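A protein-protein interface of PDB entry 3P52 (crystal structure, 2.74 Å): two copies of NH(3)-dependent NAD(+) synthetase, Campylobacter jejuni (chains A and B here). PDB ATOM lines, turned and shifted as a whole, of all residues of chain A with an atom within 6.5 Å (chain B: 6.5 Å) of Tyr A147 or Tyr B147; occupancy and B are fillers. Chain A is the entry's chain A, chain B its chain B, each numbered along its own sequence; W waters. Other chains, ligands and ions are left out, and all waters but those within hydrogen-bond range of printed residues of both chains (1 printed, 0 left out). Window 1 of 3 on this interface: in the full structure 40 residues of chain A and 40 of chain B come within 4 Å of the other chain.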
ATOM      1  N   ALA A 112      -1.834  16.531  21.461  1.00  0.00           N
ATOM      2  CA  ALA A 112      -0.405  16.466  21.443  1.00  0.00           C
ATOM      3  C   ALA A 112       0.089  15.459  22.489  1.00  0.00           C
ATOM      4  O   ALA A 112       1.056  14.757  22.214  1.00  0.00           O
ATOM      5  CB  ALA A 112       0.184  17.820  21.658  1.00  0.00           C
ATOM      6  N   ARG A 113      -0.538  15.328  23.633  1.00  0.00           N
ATOM      7  CA  ARG A 113      -0.021  14.409  24.620  1.00  0.00           C
ATOM      8  C   ARG A 113      -0.457  12.978  24.416  1.00  0.00           C
ATOM      9  O   ARG A 113       0.173  12.057  24.852  1.00  0.00           O
ATOM     10  CB  ARG A 113      -0.364  14.914  25.988  1.00  0.00           C
ATOM     11  CG  ARG A 113      -0.178  16.366  26.053  1.00  0.00           C
ATOM     12  CD  ARG A 113      -0.279  16.906  27.415  1.00  0.00           C
ATOM     13  NE  ARG A 113       0.483  18.131  27.500  1.00  0.00           N
ATOM     14  CZ  ARG A 113       0.021  19.286  27.929  1.00  0.00           C
ATOM     15  NH1 ARG A 113       0.815  20.313  27.946  1.00  0.00           N
ATOM     16  NH2 ARG A 113      -1.213  19.417  28.335  1.00  0.00           N
ATOM     17  N   ILE A 114      -1.537  12.801  23.703  1.00  0.00           N
ATOM     18  CA  ILE A 114      -1.928  11.492  23.250  1.00  0.00           C
ATOM     19  C   ILE A 114      -0.845  11.006  22.284  1.00  0.00           C
ATOM     20  O   ILE A 114      -0.334   9.888  22.404  1.00  0.00           O
ATOM     21  CB  ILE A 114      -3.329  11.521  22.579  1.00  0.00           C
ATOM     22  CG1 ILE A 114      -4.387  11.715  23.641  1.00  0.00           C
ATOM     23  CG2 ILE A 114      -3.566  10.267  21.776  1.00  0.00           C
ATOM     24  CD1 ILE A 114      -5.659  12.300  23.142  1.00  0.00           C
ATOM     25  N   MET A 116       2.225  11.819  22.254  1.00  0.00           N
ATOM     26  CA  MET A 116       3.458  11.442  22.919  1.00  0.00           C
ATOM     27  C   MET A 116       3.351  10.131  23.663  1.00  0.00           C
ATOM     28  O   MET A 116       4.263   9.321  23.584  1.00  0.00           O
ATOM     29  CB  MET A 116       4.119  12.557  23.692  1.00  0.00           C
ATOM     30  CG  MET A 116       3.707  12.736  25.055  1.00  0.00           C
ATOM     31  SD  MET A 116       4.485  11.467  26.343  1.00  0.00           S
ATOM     32  CE  MET A 116       3.113  11.897  27.684  1.00  0.00           C
ATOM     33  N   SER A 117       2.223   9.901  24.322  1.00  0.00           N
ATOM     34  CA  SER A 117       1.985   8.642  24.980  1.00  0.00           C
ATOM     35  C   SER A 117       2.040   7.455  24.039  1.00  0.00           C
ATOM     36  O   SER A 117       2.695   6.487  24.345  1.00  0.00           O
ATOM     37  CB  SER A 117       0.621   8.644  25.653  1.00  0.00           C
ATOM     38  OG  SER A 117       0.488   9.788  26.455  1.00  0.00           O
ATOM     39  N   TYR A 120       5.603   6.935  22.957  1.00  0.00           N
ATOM     40  CA  TYR A 120       6.427   6.316  24.009  1.00  0.00           C
ATOM     41  C   TYR A 120       6.097   4.860  24.204  1.00  0.00           C
ATOM     42  O   TYR A 120       7.003   4.065  24.396  1.00  0.00           O
ATOM     43  CB  TYR A 120       6.454   7.112  25.314  1.00  0.00           C
ATOM     44  CG  TYR A 120       7.585   8.138  25.263  1.00  0.00           C
ATOM     45  CD1 TYR A 120       7.407   9.374  24.618  1.00  0.00           C
ATOM     46  CD2 TYR A 120       8.842   7.841  25.798  1.00  0.00           C
ATOM     47  CE1 TYR A 120       8.474  10.298  24.537  1.00  0.00           C
ATOM     48  CE2 TYR A 120       9.905   8.731  25.724  1.00  0.00           C
ATOM     49  CZ  TYR A 120       9.734   9.964  25.095  1.00  0.00           C
ATOM     50  OH  TYR A 120      10.798  10.869  25.008  1.00  0.00           O
ATOM     51  N   THR A 145       3.522  21.969  22.807  1.00  0.00           N
ATOM     52  CA  THR A 145       2.856  21.625  24.035  1.00  0.00           C
ATOM     53  C   THR A 145       3.851  20.891  24.905  1.00  0.00           C
ATOM     54  O   THR A 145       4.471  19.937  24.444  1.00  0.00           O
ATOM     55  CB  THR A 145       1.724  20.667  23.714  1.00  0.00           C
ATOM     56  OG1 THR A 145       0.790  21.329  22.850  1.00  0.00           O
ATOM     57  CG2 THR A 145       1.076  20.159  24.979  1.00  0.00           C
ATOM     58  N   ILE A 146       4.002  21.328  26.160  1.00  0.00           N
ATOM     59  CA  ILE A 146       4.967  20.704  27.074  1.00  0.00           C
ATOM     60  C   ILE A 146       4.552  19.269  27.353  1.00  0.00           C
ATOM     61  O   ILE A 146       3.417  18.999  27.661  1.00  0.00           O
ATOM     62  CB  ILE A 146       5.107  21.450  28.426  1.00  0.00           C
ATOM     63  CG1 ILE A 146       3.764  21.926  28.951  1.00  0.00           C
ATOM     64  CG2 ILE A 146       6.003  22.641  28.316  1.00  0.00           C
ATOM     65  CD1 ILE A 146       3.916  22.597  30.300  1.00  0.00           C
ATOM     66  N   TYR A 147       5.475  18.340  27.258  1.00  0.00           N
ATOM     67  CA  TYR A 147       5.126  16.953  27.456  1.00  0.00           C
ATOM     68  C   TYR A 147       4.223  16.508  26.320  1.00  0.00           C
ATOM     69  O   TYR A 147       3.564  15.476  26.422  1.00  0.00           O
ATOM     70  CB  TYR A 147       4.473  16.723  28.837  1.00  0.00           C
ATOM     71  CG  TYR A 147       5.194  17.472  29.925  1.00  0.00           C
ATOM     72  CD1 TYR A 147       6.545  17.238  30.150  1.00  0.00           C
ATOM     73  CD2 TYR A 147       4.542  18.449  30.700  1.00  0.00           C
ATOM     74  CE1 TYR A 147       7.243  17.927  31.103  1.00  0.00           C
ATOM     75  CE2 TYR A 147       5.228  19.153  31.682  1.00  0.00           C
ATOM     76  CZ  TYR A 147       6.595  18.884  31.869  1.00  0.00           C
ATOM     77  OH  TYR A 147       7.361  19.548  32.818  1.00  0.00           O
ATOM     78  N   GLY A 148       4.209  17.306  25.251  1.00  0.00           N
ATOM     79  CA  GLY A 148       3.407  17.034  24.086  1.00  0.00           C
ATOM     80  C   GLY A 148       4.390  16.700  23.016  1.00  0.00           C
ATOM     81  O   GLY A 148       5.090  15.693  23.112  1.00  0.00           O
ATOM     82  N   ASP A 149       4.448  17.553  21.997  1.00  0.00           N
ATOM     83  CA  ASP A 149       5.427  17.417  20.917  1.00  0.00           C
ATOM     84  C   ASP A 149       6.815  17.898  21.323  1.00  0.00           C
ATOM     85  O   ASP A 149       7.788  17.696  20.600  1.00  0.00           O
ATOM     86  CB  ASP A 149       4.959  18.105  19.640  1.00  0.00           C
ATOM     87  CG  ASP A 149       4.275  19.437  19.891  1.00  0.00           C
ATOM     88  OD1 ASP A 149       4.171  20.223  18.942  1.00  0.00           O
ATOM     89  OD2 ASP A 149       3.815  19.725  21.007  1.00  0.00           O
ATOM     90  N   LEU A 150       6.922  18.535  22.481  1.00  0.00           N
ATOM     91  CA  LEU A 150       8.222  18.843  23.063  1.00  0.00           C
ATOM     92  C   LEU A 150       8.888  17.639  23.749  1.00  0.00           C
ATOM     93  O   LEU A 150      10.068  17.697  24.069  1.00  0.00           O
ATOM     94  CB  LEU A 150       8.097  20.013  24.025  1.00  0.00           C
ATOM     95  CG  LEU A 150       7.701  21.369  23.408  1.00  0.00           C
ATOM     96  CD1 LEU A 150       7.441  22.500  24.392  1.00  0.00           C
ATOM     97  CD2 LEU A 150       8.705  21.861  22.331  1.00  0.00           C
ATOM     98  N   ALA A 151       8.170  16.547  23.962  1.00  0.00           N
ATOM     99  CA  ALA A 151       8.752  15.362  24.614  1.00  0.00           C
ATOM    100  C   ALA A 151       9.498  14.490  23.611  1.00  0.00           C
ATOM    101  O   ALA A 151       8.900  14.027  22.658  1.00  0.00           O
ATOM    102  CB  ALA A 151       7.651  14.504  25.301  1.00  0.00           C
ATOM    103  N   CYS A 152      10.778  14.229  23.856  1.00  0.00           N
ATOM    104  CA  CYS A 152      11.562  13.277  23.044  1.00  0.00           C
ATOM    105  C   CYS A 152      12.918  12.990  23.709  1.00  0.00           C
ATOM    106  O   CYS A 152      13.327  13.697  24.649  1.00  0.00           O
ATOM    107  CB  CYS A 152      11.780  13.813  21.633  1.00  0.00           C
ATOM    108  SG  CYS A 152      12.846  15.346  21.540  1.00  0.00           S
ATOM    109  N   ALA A 153      13.612  11.964  23.224  1.00  0.00           N
ATOM    110  CA  ALA A 153      14.971  11.669  23.701  1.00  0.00           C
ATOM    111  C   ALA A 153      15.961  12.647  23.123  1.00  0.00           C
ATOM    112  O   ALA A 153      16.750  13.224  23.859  1.00  0.00           O
ATOM    113  CB  ALA A 153      15.388  10.268  23.387  1.00  0.00           C
ATOM    114  N   LYS A 242      13.059  24.352  30.043  1.00  0.00           N
ATOM    115  CA  LYS A 242      13.690  24.121  31.345  1.00  0.00           C
ATOM    116  C   LYS A 242      13.052  22.947  32.112  1.00  0.00           C
ATOM    117  O   LYS A 242      11.842  22.699  31.990  1.00  0.00           O
ATOM    118  CB  LYS A 242      13.636  25.413  32.188  1.00  0.00           C
ATOM    119  CG  LYS A 242      14.483  26.594  31.670  1.00  0.00           C
ATOM    120  CD  LYS A 242      14.311  27.816  32.595  1.00  0.00           C
ATOM    121  CE  LYS A 242      15.143  29.037  32.163  1.00  0.00           C
ATOM    122  NZ  LYS A 242      14.974  30.241  33.031  1.00  0.00           N
ATOM    123  N   MET A 243      13.875  22.234  32.889  1.00  0.00           N
ATOM    124  CA  MET A 243      13.408  21.194  33.821  1.00  0.00           C
ATOM    125  C   MET A 243      12.578  21.796  34.963  1.00  0.00           C
ATOM    126  O   MET A 243      12.658  23.001  35.214  1.00  0.00           O
ATOM    127  CB  MET A 243      14.601  20.465  34.437  1.00  0.00           C
ATOM    128  CG  MET A 243      15.361  19.538  33.505  1.00  0.00           C
ATOM    129  SD  MET A 243      14.405  17.868  33.049  1.00  0.00           S
ATOM    130  CE  MET A 243      14.178  17.038  34.830  1.00  0.00           C
ATOM    131  N   PRO A 244      11.788  20.964  35.669  1.00  0.00           N
ATOM    132  CA  PRO A 244      11.140  21.482  36.863  1.00  0.00           C
ATOM    133  C   PRO A 244      12.175  21.928  37.890  1.00  0.00           C
ATOM    134  O   PRO A 244      13.202  21.270  38.066  1.00  0.00           O
ATOM    135  CB  PRO A 244      10.341  20.280  37.383  1.00  0.00           C
ATOM    136  CG  PRO A 244      10.930  19.106  36.726  1.00  0.00           C
ATOM    137  CD  PRO A 244      11.355  19.587  35.384  1.00  0.00           C
ATOM    138  N   ALA B 112       0.141   7.030  34.156  1.00  0.00           N
ATOM    139  CA  ALA B 112       0.820   8.222  34.629  1.00  0.00           C
ATOM    140  C   ALA B 112       0.658   9.383  33.656  1.00  0.00           C
ATOM    141  O   ALA B 112       0.489  10.505  34.078  1.00  0.00           O
ATOM    142  CB  ALA B 112       2.281   7.957  34.925  1.00  0.00           C
ATOM    143  N   ARG B 113       0.665   9.109  32.364  1.00  0.00           N
ATOM    144  CA  ARG B 113       0.638  10.162  31.399  1.00  0.00           C
ATOM    145  C   ARG B 113      -0.758  10.705  31.181  1.00  0.00           C
ATOM    146  O   ARG B 113      -0.926  11.891  30.791  1.00  0.00           O
ATOM    147  CB  ARG B 113       1.341   9.726  30.115  1.00  0.00           C
ATOM    148  CG  ARG B 113       2.747   9.270  30.477  1.00  0.00           C
ATOM    149  CD  ARG B 113       3.790   9.353  29.426  1.00  0.00           C
ATOM    150  NE  ARG B 113       4.221   8.047  29.016  1.00  0.00           N
ATOM    151  CZ  ARG B 113       5.459   7.567  29.049  1.00  0.00           C
ATOM    152  NH1 ARG B 113       6.485   8.275  29.483  1.00  0.00           N
ATOM    153  NH2 ARG B 113       5.654   6.341  28.598  1.00  0.00           N
ATOM    154  N   ILE B 114      -1.757   9.891  31.499  1.00  0.00           N
ATOM    155  CA  ILE B 114      -3.140  10.340  31.526  1.00  0.00           C
ATOM    156  C   ILE B 114      -3.296  11.362  32.642  1.00  0.00           C
ATOM    157  O   ILE B 114      -3.828  12.475  32.448  1.00  0.00           O
ATOM    158  CB  ILE B 114      -4.110   9.119  31.713  1.00  0.00           C
ATOM    159  CG1 ILE B 114      -4.180   8.294  30.415  1.00  0.00           C
ATOM    160  CG2 ILE B 114      -5.505   9.571  32.182  1.00  0.00           C
ATOM    161  CD1 ILE B 114      -4.793   6.984  30.547  1.00  0.00           C
ATOM    162  N   MET B 116      -1.025  13.189  33.922  1.00  0.00           N
ATOM    163  CA  MET B 116      -0.359  14.453  33.686  1.00  0.00           C
ATOM    164  C   MET B 116      -1.134  15.263  32.668  1.00  0.00           C
ATOM    165  O   MET B 116      -1.204  16.475  32.800  1.00  0.00           O
ATOM    166  CB  MET B 116       1.157  14.369  33.422  1.00  0.00           C
ATOM    167  CG  MET B 116       1.560  14.103  32.015  1.00  0.00           C
ATOM    168  SD  MET B 116       1.414  15.652  30.792  1.00  0.00           S
ATOM    169  CE  MET B 116       1.324  14.607  29.168  1.00  0.00           C
ATOM    170  N   SER B 117      -1.758  14.597  31.701  1.00  0.00           N
ATOM    171  CA  SER B 117      -2.556  15.350  30.740  1.00  0.00           C
ATOM    172  C   SER B 117      -3.742  16.040  31.392  1.00  0.00           C
ATOM    173  O   SER B 117      -4.009  17.195  31.087  1.00  0.00           O
ATOM    174  CB  SER B 117      -3.045  14.462  29.637  1.00  0.00           C
ATOM    175  OG  SER B 117      -1.934  13.875  29.041  1.00  0.00           O
ATOM    176  N   TYR B 120      -2.496  18.941  33.370  1.00  0.00           N
ATOM    177  CA  TYR B 120      -2.148  20.090  32.578  1.00  0.00           C
ATOM    178  C   TYR B 120      -3.366  20.826  32.017  1.00  0.00           C
ATOM    179  O   TYR B 120      -3.406  22.070  32.008  1.00  0.00           O
ATOM    180  CB  TYR B 120      -1.064  19.771  31.590  1.00  0.00           C
ATOM    181  CG  TYR B 120       0.280  20.014  32.250  1.00  0.00           C
ATOM    182  CD1 TYR B 120       0.885  19.054  33.050  1.00  0.00           C
ATOM    183  CD2 TYR B 120       0.939  21.230  32.099  1.00  0.00           C
ATOM    184  CE1 TYR B 120       2.094  19.293  33.647  1.00  0.00           C
ATOM    185  CE2 TYR B 120       2.120  21.470  32.701  1.00  0.00           C
ATOM    186  CZ  TYR B 120       2.694  20.497  33.475  1.00  0.00           C
ATOM    187  OH  TYR B 120       3.895  20.776  34.080  1.00  0.00           O
ATOM    188  N   THR B 145       7.556   7.823  35.752  1.00  0.00           N
ATOM    189  CA  THR B 145       7.404   7.807  34.299  1.00  0.00           C
ATOM    190  C   THR B 145       7.776   9.162  33.711  1.00  0.00           C
ATOM    191  O   THR B 145       7.271  10.211  34.178  1.00  0.00           O
ATOM    192  CB  THR B 145       5.958   7.637  33.976  1.00  0.00           C
ATOM    193  OG1 THR B 145       5.502   6.445  34.590  1.00  0.00           O
ATOM    194  CG2 THR B 145       5.752   7.577  32.510  1.00  0.00           C
ATOM    195  N   ILE B 146       8.628   9.162  32.682  1.00  0.00           N
ATOM    196  CA  ILE B 146       8.966  10.430  32.046  1.00  0.00           C
ATOM    197  C   ILE B 146       7.728  11.019  31.434  1.00  0.00           C
ATOM    198  O   ILE B 146       6.980  10.299  30.812  1.00  0.00           O
ATOM    199  CB  ILE B 146      10.024  10.314  30.941  1.00  0.00           C
ATOM    200  CG1 ILE B 146       9.852   9.041  30.131  1.00  0.00           C
ATOM    201  CG2 ILE B 146      11.435  10.423  31.514  1.00  0.00           C
ATOM    202  CD1 ILE B 146      10.897   8.952  29.032  1.00  0.00           C
ATOM    203  N   TYR B 147       7.519  12.325  31.608  1.00  0.00           N
ATOM    204  CA  TYR B 147       6.357  12.998  31.064  1.00  0.00           C
ATOM    205  C   TYR B 147       5.079  12.450  31.673  1.00  0.00           C
ATOM    206  O   TYR B 147       4.010  12.677  31.133  1.00  0.00           O
ATOM    207  CB  TYR B 147       6.314  12.859  29.540  1.00  0.00           C
ATOM    208  CG  TYR B 147       7.642  13.110  28.893  1.00  0.00           C
ATOM    209  CD1 TYR B 147       8.303  14.313  29.102  1.00  0.00           C
ATOM    210  CD2 TYR B 147       8.258  12.137  28.081  1.00  0.00           C
ATOM    211  CE1 TYR B 147       9.532  14.558  28.526  1.00  0.00           C
ATOM    212  CE2 TYR B 147       9.509  12.378  27.502  1.00  0.00           C
ATOM    213  CZ  TYR B 147      10.129  13.598  27.735  1.00  0.00           C
ATOM    214  OH  TYR B 147      11.337  13.911  27.191  1.00  0.00           O
ATOM    215  N   GLY B 148       5.215  11.708  32.773  1.00  0.00           N
ATOM    216  CA  GLY B 148       4.096  11.198  33.561  1.00  0.00           C
ATOM    217  C   GLY B 148       4.116  11.955  34.871  1.00  0.00           C
ATOM    218  O   GLY B 148       3.922  13.145  34.879  1.00  0.00           O
ATOM    219  N   ASP B 149       4.403  11.283  35.981  1.00  0.00           N
ATOM    220  CA  ASP B 149       4.525  11.953  37.296  1.00  0.00           C
ATOM    221  C   ASP B 149       5.804  12.749  37.471  1.00  0.00           C
ATOM    222  O   ASP B 149       5.957  13.467  38.456  1.00  0.00           O
ATOM    223  CB  ASP B 149       4.353  10.973  38.463  1.00  0.00           C
ATOM    224  CG  ASP B 149       5.030   9.601  38.224  1.00  0.00           C
ATOM    225  OD1 ASP B 149       5.286   8.917  39.226  1.00  0.00           O
ATOM    226  OD2 ASP B 149       5.294   9.170  37.065  1.00  0.00           O
ATOM    227  N   LEU B 150       6.719  12.639  36.519  1.00  0.00           N
ATOM    228  CA  LEU B 150       7.890  13.506  36.501  1.00  0.00           C
ATOM    229  C   LEU B 150       7.597  14.919  35.933  1.00  0.00           C
ATOM    230  O   LEU B 150       8.400  15.834  36.104  1.00  0.00           O
ATOM    231  CB  LEU B 150       9.034  12.808  35.764  1.00  0.00           C
ATOM    232  CG  LEU B 150       9.636  11.515  36.381  1.00  0.00           C
ATOM    233  CD1 LEU B 150      10.669  10.811  35.508  1.00  0.00           C
ATOM    234  CD2 LEU B 150      10.202  11.694  37.795  1.00  0.00           C
ATOM    235  N   ALA B 151       6.442  15.111  35.303  1.00  0.00           N
ATOM    236  CA  ALA B 151       6.140  16.373  34.626  1.00  0.00           C
ATOM    237  C   ALA B 151       5.485  17.354  35.577  1.00  0.00           C
ATOM    238  O   ALA B 151       4.427  17.071  36.099  1.00  0.00           O
ATOM    239  CB  ALA B 151       5.219  16.131  33.452  1.00  0.00           C
ATOM    240  N   CYS B 152       6.112  18.507  35.778  1.00  0.00           N
ATOM    241  CA  CYS B 152       5.532  19.557  36.587  1.00  0.00           C
ATOM    242  C   CYS B 152       6.280  20.866  36.336  1.00  0.00           C
ATOM    243  O   CYS B 152       7.330  20.838  35.719  1.00  0.00           O
ATOM    244  CB  CYS B 152       5.563  19.183  38.071  1.00  0.00           C
ATOM    245  SG  CYS B 152       7.210  18.948  38.746  1.00  0.00           S
ATOM    246  N   ALA B 153       5.740  21.996  36.801  1.00  0.00           N
ATOM    247  CA  ALA B 153       6.445  23.286  36.750  1.00  0.00           C
ATOM    248  C   ALA B 153       7.564  23.365  37.799  1.00  0.00           C
ATOM    249  O   ALA B 153       8.676  23.792  37.496  1.00  0.00           O
ATOM    250  CB  ALA B 153       5.476  24.439  36.918  1.00  0.00           C
ATOM    251  N   LYS B 242      17.219  14.808  32.765  1.00  0.00           N
ATOM    252  CA  LYS B 242      17.868  15.598  31.698  1.00  0.00           C
ATOM    253  C   LYS B 242      16.903  15.971  30.549  1.00  0.00           C
ATOM    254  O   LYS B 242      15.992  15.214  30.215  1.00  0.00           O
ATOM    255  CB  LYS B 242      19.090  14.838  31.135  1.00  0.00           C
ATOM    256  CG  LYS B 242      20.273  14.658  32.100  1.00  0.00           C
ATOM    257  CD  LYS B 242      21.468  13.976  31.402  1.00  0.00           C
ATOM    258  CE  LYS B 242      22.726  13.883  32.295  1.00  0.00           C
ATOM    259  NZ  LYS B 242      22.599  12.905  33.409  1.00  0.00           N
ATOM    260  N   MET B 243      17.114  17.145  29.956  1.00  0.00           N
ATOM    261  CA  MET B 243      16.385  17.586  28.764  1.00  0.00           C
ATOM    262  C   MET B 243      16.815  16.785  27.546  1.00  0.00           C
ATOM    263  O   MET B 243      17.887  16.172  27.546  1.00  0.00           O
ATOM    264  CB  MET B 243      16.704  19.053  28.473  1.00  0.00           C
ATOM    265  CG  MET B 243      16.103  20.052  29.441  1.00  0.00           C
ATOM    266  SD  MET B 243      14.161  20.300  29.203  1.00  0.00           S
ATOM    267  CE  MET B 243      14.119  20.996  27.350  1.00  0.00           C
ATOM    268  N   PRO B 244      15.996  16.806  26.487  1.00  0.00           N
ATOM    269  CA  PRO B 244      16.441  16.182  25.260  1.00  0.00           C
ATOM    270  C   PRO B 244      17.702  16.837  24.729  1.00  0.00           C
ATOM    271  O   PRO B 244      17.825  18.058  24.775  1.00  0.00           O
ATOM    272  CB  PRO B 244      15.277  16.431  24.301  1.00  0.00           C
ATOM    273  CG  PRO B 244      14.491  17.514  24.914  1.00  0.00           C
ATOM    274  CD  PRO B 244      14.619  17.303  26.371  1.00  0.00           C
HETATM  275  O   HOH W   1       7.817   4.399  27.676  1.00  0.00           O
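OH of Tyr A147 sits at hydrogen-bond distance from O of Cys B152, 3.2 Å away.
OH of Tyr B147 is in hydrogen-bond range of O of Cys A152, at 3.2 Å.
The backbone carbonyl oxygen (O) of Arg A113 lies within hydrogen-bond range of the side-chain hydroxyl (OG) of Ser A117, at 2.8 Å.
The guanidinium group of Arg A113 sits at hydrogen-bond distance from the backbone carbonyl oxygen of Ile A146, at 2.9 Å.
O of Arg B113 sits at hydrogen-bond distance from OG of Ser B117, at 2.8 Å.
NH1 of Arg B113 is in hydrogen-bond range of O of Ile B146 (2.5 Å).
Among the printed residues, merely in contact across the chains: Arg A113 with Met B116 (3.3 Å), Arg A113 with Ser B117 (3.6 Å), Arg A113 with Tyr B120 (3.3 Å), Met A116 with Arg B113 (3.2 Å), Met A116 with Met B116 (3.6 Å), Met A116 with Tyr B147 (3.6 Å), Ser A117 with Arg B113 (3.8 Å), Tyr A120 with Arg B113 (3.5 Å), Tyr A120 with Ile B146 (3.5 Å), Tyr A120 with Tyr B147 (3.2 Å), Ile A146 with Tyr B120 (3.2 Å), Tyr A147 with Met B116 (3.6 Å), Tyr A147 with Tyr B120 (3.2 Å), Tyr A147 with Tyr B147 (3.6 Å), Tyr A147 with Ala B151 (3.5 Å), Ala A151 with Tyr B147 (3.6 Å), Cys A152 with Pro B244 (3.4 Å), Ala A153 with Pro B244 (3.3 Å), Pro A244 with Cys B152 (3.5 Å) and Pro A244 with Ala B153 (3.4 Å).
Tyr A147 touches just these residues of chain B: Met B116 (3.6 Å), Tyr B120 (3.2 Å), Tyr B147 (3.6 Å), Ala B151 (3.5 Å) and Cys B152 (3.2 Å).
Of chain A, only Met A116, Tyr A120, Tyr A147, Ala A151 and Cys A152 come within 4 Å of Tyr B147.
Of the printed residues of chain B, Ile A146 touches Tyr B120.
Of the printed residues of chain B, Ala A151 touches Tyr B147 (3.6 Å).
Of the printed residues of chain A, Cys B152 touches Tyr A147 (3.2 Å) and Pro A244 (3.5 Å).
Of the printed residues of chain A, Ser B117 touches Arg A113.
The nearest residue of chain B that does not touch Tyr A147 is Ala B153 (4.9 Å).
The nearest residue of chain A that does not touch Tyr B147 is Ala A153 (5.0 Å).
The nearest printed residue of chain B that does not touch Arg A113 is Arg B113 (5.7 Å).
Printed residues of chain B that touch a printed residue of chain A: Arg B113, Met B116, Ser B117, Tyr B120, Ile B146, Tyr B147, Ala B151, Cys B152, Ala B153 and Pro B244.
Hydrophobic or aromatic side chains of chain B within 4 Å of the printed part of chain A: Met B116, Tyr B120, Ile B146, Tyr B147, Ala B151 and Pro B244.
Among the printed residues, no Asp or Glu carboxylate lies within 4 Å of a Lys or Arg side-chain nitrogen of the other chain.
Arg A113 touches Met B116, and with the chains exchanged Met A116 touches Arg B113.
Arg A113 touches Ser B117, and with the chains exchanged Ser A117 touches Arg B113.
Tyr A147 touches Cys B152, and with the chains exchanged Cys A152 touches Tyr B147.
Cys A152 touches Pro B244, and with the chains exchanged Pro A244 touches Cys B152.
Of the 22 pairs that touch across the chains among the printed residues, 22 have their exchanged pair printed and touching as well.
Water W1 lies within hydrogen-bond range of NH2 of Arg B113 (3.0 Å) and O of Tyr A120 (3.4 Å).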
